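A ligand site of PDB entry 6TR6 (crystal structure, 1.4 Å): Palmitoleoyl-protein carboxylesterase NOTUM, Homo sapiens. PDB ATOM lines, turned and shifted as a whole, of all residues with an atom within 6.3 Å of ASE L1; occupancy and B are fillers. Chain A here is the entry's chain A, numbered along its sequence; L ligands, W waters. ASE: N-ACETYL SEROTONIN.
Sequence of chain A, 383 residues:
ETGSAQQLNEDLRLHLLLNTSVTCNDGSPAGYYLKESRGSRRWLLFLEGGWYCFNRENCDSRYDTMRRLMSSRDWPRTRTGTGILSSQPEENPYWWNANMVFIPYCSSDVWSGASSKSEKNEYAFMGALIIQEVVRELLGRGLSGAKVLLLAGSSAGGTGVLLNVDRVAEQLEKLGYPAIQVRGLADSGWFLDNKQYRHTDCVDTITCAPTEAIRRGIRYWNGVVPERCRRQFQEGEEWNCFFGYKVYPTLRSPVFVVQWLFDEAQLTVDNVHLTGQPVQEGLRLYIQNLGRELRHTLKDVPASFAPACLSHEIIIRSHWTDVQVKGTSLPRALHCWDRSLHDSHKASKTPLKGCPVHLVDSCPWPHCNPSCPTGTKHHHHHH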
ATOM      1  N   GLY A  50       2.947 -18.681 -12.588  1.00  0.00           N
ATOM      2  CA  GLY A  50       2.091 -17.932 -11.667  1.00  0.00           C
ATOM      3  C   GLY A  50       2.122 -18.406 -10.225  1.00  0.00           C
ATOM      4  O   GLY A  50       1.061 -18.630  -9.617  1.00  0.00           O
ATOM      5  N   TRP A  51       3.303 -18.562  -9.656  1.00  0.00           N
ATOM      6  CA  TRP A  51       3.520 -18.929  -8.244  1.00  0.00           C
ATOM      7  C   TRP A  51       2.833 -20.266  -7.957  1.00  0.00           C
ATOM      8  O   TRP A  51       2.905 -21.170  -8.800  1.00  0.00           O
ATOM      9  CB  TRP A  51       3.163 -17.769  -7.327  1.00  0.00           C
ATOM     10  CG  TRP A  51       4.114 -16.623  -7.499  1.00  0.00           C
ATOM     11  CD1 TRP A  51       3.950 -15.544  -8.308  1.00  0.00           C
ATOM     12  CD2 TRP A  51       5.396 -16.469  -6.871  1.00  0.00           C
ATOM     13  NE1 TRP A  51       5.041 -14.713  -8.212  1.00  0.00           N
ATOM     14  CE2 TRP A  51       5.946 -15.252  -7.347  1.00  0.00           C
ATOM     15  CE3 TRP A  51       6.132 -17.230  -5.955  1.00  0.00           C
ATOM     16  CZ2 TRP A  51       7.194 -14.781  -6.921  1.00  0.00           C
ATOM     17  CZ3 TRP A  51       7.365 -16.763  -5.548  1.00  0.00           C
ATOM     18  CH2 TRP A  51       7.882 -15.547  -6.028  1.00  0.00           C
ATOM     19  N   TYR A  52       2.216 -20.436  -6.788  1.00  0.00           N
ATOM     20  CA  TYR A  52       1.661 -21.712  -6.350  1.00  0.00           C
ATOM     21  C   TYR A  52       0.935 -21.417  -5.040  1.00  0.00           C
ATOM     22  O   TYR A  52       1.016 -20.314  -4.508  1.00  0.00           O
ATOM     23  CB  TYR A  52       2.742 -22.797  -6.166  1.00  0.00           C
ATOM     24  CG  TYR A  52       3.838 -22.446  -5.187  1.00  0.00           C
ATOM     25  CD1 TYR A  52       3.734 -22.824  -3.852  1.00  0.00           C
ATOM     26  CD2 TYR A  52       4.989 -21.775  -5.593  1.00  0.00           C
ATOM     27  CE1 TYR A  52       4.730 -22.517  -2.930  1.00  0.00           C
ATOM     28  CE2 TYR A  52       6.010 -21.470  -4.669  1.00  0.00           C
ATOM     29  CZ  TYR A  52       5.859 -21.837  -3.350  1.00  0.00           C
ATOM     30  OH  TYR A  52       6.849 -21.543  -2.426  1.00  0.00           O
ATOM     31  N   VAL A 110       3.297 -25.914  -9.230  1.00  0.00           N
ATOM     32  CA  VAL A 110       4.525 -25.882 -10.022  1.00  0.00           C
ATOM     33  C   VAL A 110       4.549 -27.050 -11.023  1.00  0.00           C
ATOM     34  O   VAL A 110       5.607 -27.580 -11.368  1.00  0.00           O
ATOM     35  CB  VAL A 110       5.799 -25.838  -9.140  1.00  0.00           C
ATOM     36  CG1 VAL A 110       6.997 -25.352  -9.960  1.00  0.00           C
ATOM     37  CG2 VAL A 110       5.595 -24.911  -7.944  1.00  0.00           C
ATOM     38  N   SER A 155       8.695 -19.119 -15.543  1.00  0.00           N
ATOM     39  CA  SER A 155       8.508 -18.931 -14.094  1.00  0.00           C
ATOM     40  C   SER A 155       8.141 -20.269 -13.476  1.00  0.00           C
ATOM     41  O   SER A 155       8.915 -21.225 -13.619  1.00  0.00           O
ATOM     42  CB  SER A 155       7.540 -17.770 -13.857  1.00  0.00           C
ATOM     43  OG  SER A 155       7.892 -16.624 -14.632  1.00  0.00           O
ATOM     44  N   ALA A 156       6.997 -20.408 -12.778  1.00  0.00           N
ATOM     45  CA  ALA A 156       6.613 -21.734 -12.317  1.00  0.00           C
ATOM     46  C   ALA A 156       6.548 -22.724 -13.481  1.00  0.00           C
ATOM     47  O   ALA A 156       6.830 -23.915 -13.294  1.00  0.00           O
ATOM     48  CB  ALA A 156       5.278 -21.687 -11.576  1.00  0.00           C
ATOM     49  N   GLY A 157       6.172 -22.249 -14.671  1.00  0.00           N
ATOM     50  CA  GLY A 157       6.205 -23.106 -15.850  1.00  0.00           C
ATOM     51  C   GLY A 157       7.608 -23.507 -16.285  1.00  0.00           C
ATOM     52  O   GLY A 157       7.791 -24.585 -16.848  1.00  0.00           O
ATOM     53  N   THR A 159      10.181 -24.020 -14.115  1.00  0.00           N
ATOM     54  CA  THR A 159      10.467 -25.150 -13.235  1.00  0.00           C
ATOM     55  C   THR A 159       9.653 -26.370 -13.654  1.00  0.00           C
ATOM     56  O   THR A 159      10.155 -27.500 -13.640  1.00  0.00           O
ATOM     57  CB  THR A 159      10.180 -24.776 -11.779  1.00  0.00           C
ATOM     58  OG1 THR A 159      10.888 -23.564 -11.458  1.00  0.00           O
ATOM     59  CG2 THR A 159      10.646 -25.882 -10.841  1.00  0.00           C
ATOM     60  N   GLY A 160       8.400 -26.142 -14.074  1.00  0.00           N
ATOM     61  CA  GLY A 160       7.568 -27.221 -14.594  1.00  0.00           C
ATOM     62  C   GLY A 160       8.206 -27.982 -15.741  1.00  0.00           C
ATOM     63  O   GLY A 160       8.094 -29.206 -15.812  1.00  0.00           O
ATOM     64  N   SER A 188      13.160 -18.628 -16.710  1.00  0.00           N
ATOM     65  CA  SER A 188      12.879 -17.951 -15.444  1.00  0.00           C
ATOM     66  C   SER A 188      12.404 -18.910 -14.353  1.00  0.00           C
ATOM     67  O   SER A 188      11.657 -18.518 -13.449  1.00  0.00           O
ATOM     68  CB  SER A 188      11.907 -16.781 -15.630  1.00  0.00           C
ATOM     69  OG  SER A 188      12.464 -15.831 -16.555  1.00  0.00           O
ATOM     70  N   GLY A 189      12.852 -20.162 -14.414  1.00  0.00           N
ATOM     71  CA  GLY A 189      12.499 -21.149 -13.404  1.00  0.00           C
ATOM     72  C   GLY A 189      13.698 -21.793 -12.752  1.00  0.00           C
ATOM     73  O   GLY A 189      13.576 -22.890 -12.200  1.00  0.00           O
ATOM     74  N   PHE A 191      16.189 -21.291  -9.895  1.00  0.00           N
ATOM     75  CA  PHE A 191      16.340 -20.524  -8.670  1.00  0.00           C
ATOM     76  C   PHE A 191      17.446 -21.096  -7.795  1.00  0.00           C
ATOM     77  O   PHE A 191      17.842 -22.257  -7.918  1.00  0.00           O
ATOM     78  CB  PHE A 191      15.009 -20.499  -7.906  1.00  0.00           C
ATOM     79  CG  PHE A 191      13.917 -19.854  -8.683  1.00  0.00           C
ATOM     80  CD1 PHE A 191      12.857 -20.589  -9.158  1.00  0.00           C
ATOM     81  CD2 PHE A 191      14.006 -18.514  -9.002  1.00  0.00           C
ATOM     82  CE1 PHE A 191      11.861 -19.990  -9.904  1.00  0.00           C
ATOM     83  CE2 PHE A 191      13.020 -17.905  -9.759  1.00  0.00           C
ATOM     84  CZ  PHE A 191      11.945 -18.647 -10.215  1.00  0.00           C
ATOM     85  N   LEU A 192      17.912 -20.263  -6.876  1.00  0.00           N
ATOM     86  CA  LEU A 192      18.923 -20.642  -5.901  1.00  0.00           C
ATOM     87  C   LEU A 192      18.290 -20.722  -4.525  1.00  0.00           C
ATOM     88  O   LEU A 192      17.530 -19.825  -4.137  1.00  0.00           O
ATOM     89  CB  LEU A 192      20.042 -19.590  -5.854  1.00  0.00           C
ATOM     90  CG  LEU A 192      20.749 -19.340  -7.188  1.00  0.00           C
ATOM     91  CD1 LEU A 192      21.836 -18.311  -6.994  1.00  0.00           C
ATOM     92  CD2 LEU A 192      21.325 -20.645  -7.734  1.00  0.00           C
ATOM     93  N   PRO A 210      10.935 -20.025   1.008  1.00  0.00           N
ATOM     94  CA  PRO A 210      10.463 -20.824  -0.142  1.00  0.00           C
ATOM     95  C   PRO A 210      10.703 -22.309  -0.002  1.00  0.00           C
ATOM     96  O   PRO A 210       9.841 -23.107  -0.411  1.00  0.00           O
ATOM     97  CB  PRO A 210      11.253 -20.246  -1.313  1.00  0.00           C
ATOM     98  CG  PRO A 210      11.518 -18.844  -0.937  1.00  0.00           C
ATOM     99  CD  PRO A 210      11.644 -18.800   0.574  1.00  0.00           C
ATOM    100  N   THR A 211      11.865 -22.722   0.528  1.00  0.00           N
ATOM    101  CA  THR A 211      12.125 -24.148   0.655  1.00  0.00           C
ATOM    102  C   THR A 211      11.107 -24.809   1.565  1.00  0.00           C
ATOM    103  O   THR A 211      10.643 -25.921   1.269  1.00  0.00           O
ATOM    104  CB  THR A 211      13.552 -24.406   1.128  1.00  0.00           C
ATOM    105  OG1 THR A 211      13.777 -23.760   2.391  1.00  0.00           O
ATOM    106  CG2 THR A 211      14.568 -23.897   0.099  1.00  0.00           C
ATOM    107  N   ILE A 214       7.723 -24.897  -0.365  1.00  0.00           N
ATOM    108  CA  ILE A 214       7.775 -25.978  -1.338  1.00  0.00           C
ATOM    109  C   ILE A 214       7.668 -27.341  -0.649  1.00  0.00           C
ATOM    110  O   ILE A 214       6.939 -28.230  -1.109  1.00  0.00           O
ATOM    111  CB  ILE A 214       9.027 -25.865  -2.233  1.00  0.00           C
ATOM    112  CG1 ILE A 214       8.884 -24.688  -3.201  1.00  0.00           C
ATOM    113  CG2 ILE A 214       9.247 -27.158  -3.048  1.00  0.00           C
ATOM    114  CD1 ILE A 214       7.769 -24.854  -4.203  1.00  0.00           C
ATOM    115  N   PHE A 242      13.174 -29.115  -7.091  1.00  0.00           N
ATOM    116  CA  PHE A 242      12.574 -27.903  -7.616  1.00  0.00           C
ATOM    117  C   PHE A 242      13.623 -26.830  -7.911  1.00  0.00           C
ATOM    118  O   PHE A 242      13.275 -25.762  -8.441  1.00  0.00           O
ATOM    119  CB  PHE A 242      11.524 -27.349  -6.645  1.00  0.00           C
ATOM    120  CG  PHE A 242      10.224 -28.089  -6.669  1.00  0.00           C
ATOM    121  CD1 PHE A 242      10.152 -29.431  -6.363  1.00  0.00           C
ATOM    122  CD2 PHE A 242       9.039 -27.409  -6.971  1.00  0.00           C
ATOM    123  CE1 PHE A 242       8.930 -30.098  -6.389  1.00  0.00           C
ATOM    124  CE2 PHE A 242       7.826 -28.071  -6.994  1.00  0.00           C
ATOM    125  CZ  PHE A 242       7.773 -29.410  -6.716  1.00  0.00           C
ATOM    126  N   PHE A 243      14.877 -27.098  -7.582  1.00  0.00           N
ATOM    127  CA  PHE A 243      15.961 -26.166  -7.827  1.00  0.00           C
ATOM    128  C   PHE A 243      16.737 -26.626  -9.058  1.00  0.00           C
ATOM    129  O   PHE A 243      17.307 -27.719  -9.061  1.00  0.00           O
ATOM    130  CB  PHE A 243      16.819 -25.985  -6.581  1.00  0.00           C
ATOM    131  CG  PHE A 243      16.111 -25.193  -5.529  1.00  0.00           C
ATOM    132  CD1 PHE A 243      15.210 -25.799  -4.677  1.00  0.00           C
ATOM    133  CD2 PHE A 243      16.247 -23.815  -5.495  1.00  0.00           C
ATOM    134  CE1 PHE A 243      14.505 -25.054  -3.749  1.00  0.00           C
ATOM    135  CE2 PHE A 243      15.547 -23.061  -4.555  1.00  0.00           C
ATOM    136  CZ  PHE A 243      14.673 -23.678  -3.697  1.00  0.00           C
ATOM    137  N   ASP A 263      17.134 -12.190 -11.261  1.00  0.00           N
ATOM    138  CA  ASP A 263      15.717 -12.434 -11.482  1.00  0.00           C
ATOM    139  C   ASP A 263      14.887 -11.811 -10.354  1.00  0.00           C
ATOM    140  O   ASP A 263      15.221 -11.932  -9.172  1.00  0.00           O
ATOM    141  CB  ASP A 263      15.484 -13.935 -11.565  1.00  0.00           C
ATOM    142  CG  ASP A 263      14.070 -14.287 -11.765  1.00  0.00           C
ATOM    143  OD1 ASP A 263      13.639 -14.353 -12.923  1.00  0.00           O
ATOM    144  OD2 ASP A 263      13.363 -14.465 -10.746  1.00  0.00           O
ATOM    145  N   ALA A 265      11.908 -12.487  -9.189  1.00  0.00           N
ATOM    146  CA  ALA A 265      11.305 -13.429  -8.242  1.00  0.00           C
ATOM    147  C   ALA A 265      12.335 -13.947  -7.249  1.00  0.00           C
ATOM    148  O   ALA A 265      12.042 -14.077  -6.061  1.00  0.00           O
ATOM    149  CB  ALA A 265      10.635 -14.580  -8.984  1.00  0.00           C
ATOM    150  N   GLN A 266      13.552 -14.234  -7.729  1.00  0.00           N
ATOM    151  CA  GLN A 266      14.642 -14.607  -6.834  1.00  0.00           C
ATOM    152  C   GLN A 266      14.897 -13.515  -5.816  1.00  0.00           C
ATOM    153  O   GLN A 266      14.972 -13.775  -4.615  1.00  0.00           O
ATOM    154  CB  GLN A 266      15.901 -14.879  -7.668  1.00  0.00           C
ATOM    155  CG  GLN A 266      17.118 -15.246  -6.818  1.00  0.00           C
ATOM    156  CD  GLN A 266      17.087 -16.689  -6.357  1.00  0.00           C
ATOM    157  OE1 GLN A 266      16.876 -17.592  -7.154  1.00  0.00           O
ATOM    158  NE2 GLN A 266      17.284 -16.903  -5.064  1.00  0.00           N
ATOM    159  N   VAL A 269      12.052 -13.262  -3.069  1.00  0.00           N
ATOM    160  CA  VAL A 269      12.106 -14.257  -2.004  1.00  0.00           C
ATOM    161  C   VAL A 269      13.370 -14.116  -1.177  1.00  0.00           C
ATOM    162  O   VAL A 269      13.416 -14.585  -0.028  1.00  0.00           O
ATOM    163  CB  VAL A 269      11.863 -15.673  -2.543  1.00  0.00           C
ATOM    164  CG1 VAL A 269      10.538 -15.685  -3.274  1.00  0.00           C
ATOM    165  CG2 VAL A 269      13.026 -16.161  -3.423  1.00  0.00           C
HETATM  166  C1  ASE L   1       8.102 -20.548  -7.873  1.00  0.00           C
HETATM  167  C2  ASE L   1       8.996 -20.838  -6.861  1.00  0.00           C
HETATM  168  C3  ASE L   1       9.947 -21.864  -7.041  1.00  0.00           C
HETATM  169  C4  ASE L   1       8.139 -21.268  -9.068  1.00  0.00           C
HETATM  170  C5  ASE L   1       9.078 -22.279  -9.236  1.00  0.00           C
HETATM  171  C6  ASE L   1       9.995 -22.577  -8.210  1.00  0.00           C
HETATM  172  C7  ASE L   1      10.968 -22.387  -6.241  1.00  0.00           C
HETATM  173  C8  ASE L   1      11.591 -23.402  -6.938  1.00  0.00           C
HETATM  174  N9  ASE L   1      10.998 -23.485  -8.112  1.00  0.00           N
HETATM  175  O10 ASE L   1       7.168 -19.540  -7.713  1.00  0.00           O
HETATM  176  C11 ASE L   1      11.323 -21.909  -4.845  1.00  0.00           C
HETATM  177  C12 ASE L   1      12.414 -20.837  -4.892  1.00  0.00           C
HETATM  178  N13 ASE L   1      12.107 -19.798  -5.854  1.00  0.00           N
HETATM  179  C14 ASE L   1      11.171 -18.765  -5.503  1.00  0.00           C
HETATM  180  C15 ASE L   1      10.848 -17.671  -6.506  1.00  0.00           C
HETATM  181  O16 ASE L   1      10.666 -18.769  -4.449  1.00  0.00           O
HETATM  182  C1  ASE L   2      21.204 -20.956   4.079  1.00  0.00           C
HETATM  183  C2  ASE L   2      20.125 -21.051   3.221  1.00  0.00           C
HETATM  184  C3  ASE L   2      18.919 -21.616   3.699  1.00  0.00           C
HETATM  185  C4  ASE L   2      21.126 -21.413   5.387  1.00  0.00           C
HETATM  186  C5  ASE L   2      19.950 -21.978   5.845  1.00  0.00           C
HETATM  187  C6  ASE L   2      18.830 -22.079   4.980  1.00  0.00           C
HETATM  188  C7  ASE L   2      17.670 -21.856   3.110  1.00  0.00           C
HETATM  189  C8  ASE L   2      16.855 -22.454   4.050  1.00  0.00           C
HETATM  190  N9  ASE L   2      17.572 -22.576   5.167  1.00  0.00           N
HETATM  191  O10 ASE L   2      22.396 -20.397   3.619  1.00  0.00           O
HETATM  192  C11 ASE L   2      17.284 -21.494   1.686  1.00  0.00           C
HETATM  193  C12 ASE L   2      16.693 -20.095   1.734  1.00  0.00           C
HETATM  194  N13 ASE L   2      16.625 -19.471   0.428  1.00  0.00           N
HETATM  195  C14 ASE L   2      15.435 -19.638  -0.363  1.00  0.00           C
HETATM  196  C15 ASE L   2      15.359 -18.966  -1.727  1.00  0.00           C
HETATM  197  O16 ASE L   2      14.545 -20.294   0.039  1.00  0.00           O
HETATM  198  O   HOH W   1       8.613 -19.479  -3.083  1.00  0.00           O
HETATM  199  O   HOH W   2       8.440 -17.875  -9.797  1.00  0.00           O
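Merely in contact with ASE L1: Trp 51 (3.1 Å), Tyr 52 (3.8 Å), Val 110 (3.8 Å), Ala 156 (3.6 Å), Phe 191 (3.4 Å), Pro 210 (3.5 Å), Phe 243 (3.8 Å), Ala 265 (3.8 Å) and Val 269 (3.3 Å). Hydrophobic or aromatic side chains that line ASE L1: Trp 51, Tyr 52, Val 110, Ala 156, Phe 191, Pro 210, Phe 242, Phe 243, Ala 265 and Val 269. Within 4 Å of ASE L1: Trp 51, Tyr 52, Val 110, Ala 156, Thr 159, Phe 191, Pro 210, Phe 242, Phe 243, Ala 265 and Val 269. The nearest printed residue that does not touch ASE L1 is Ile 214 (4.05 Å).
The side-chain hydroxyl (OG1) of Thr 159 is in hydrogen-bond range of the backbone carbonyl oxygen (O) of Gly 189. The backbone NH of Ala 265 is in hydrogen-bond range of the side-chain carboxylate of Asp 263 (2.9 Å).
A nitrogen (N9) of ASE L1 lies close to the side-chain hydroxyl (OG1) of Thr 159. O of Phe 242 sits at hydrogen-bond distance from N9 of ASE L1, at 3.2 Å.
Water W1 bridges O16 of ASE L1 and OH of Tyr 52.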
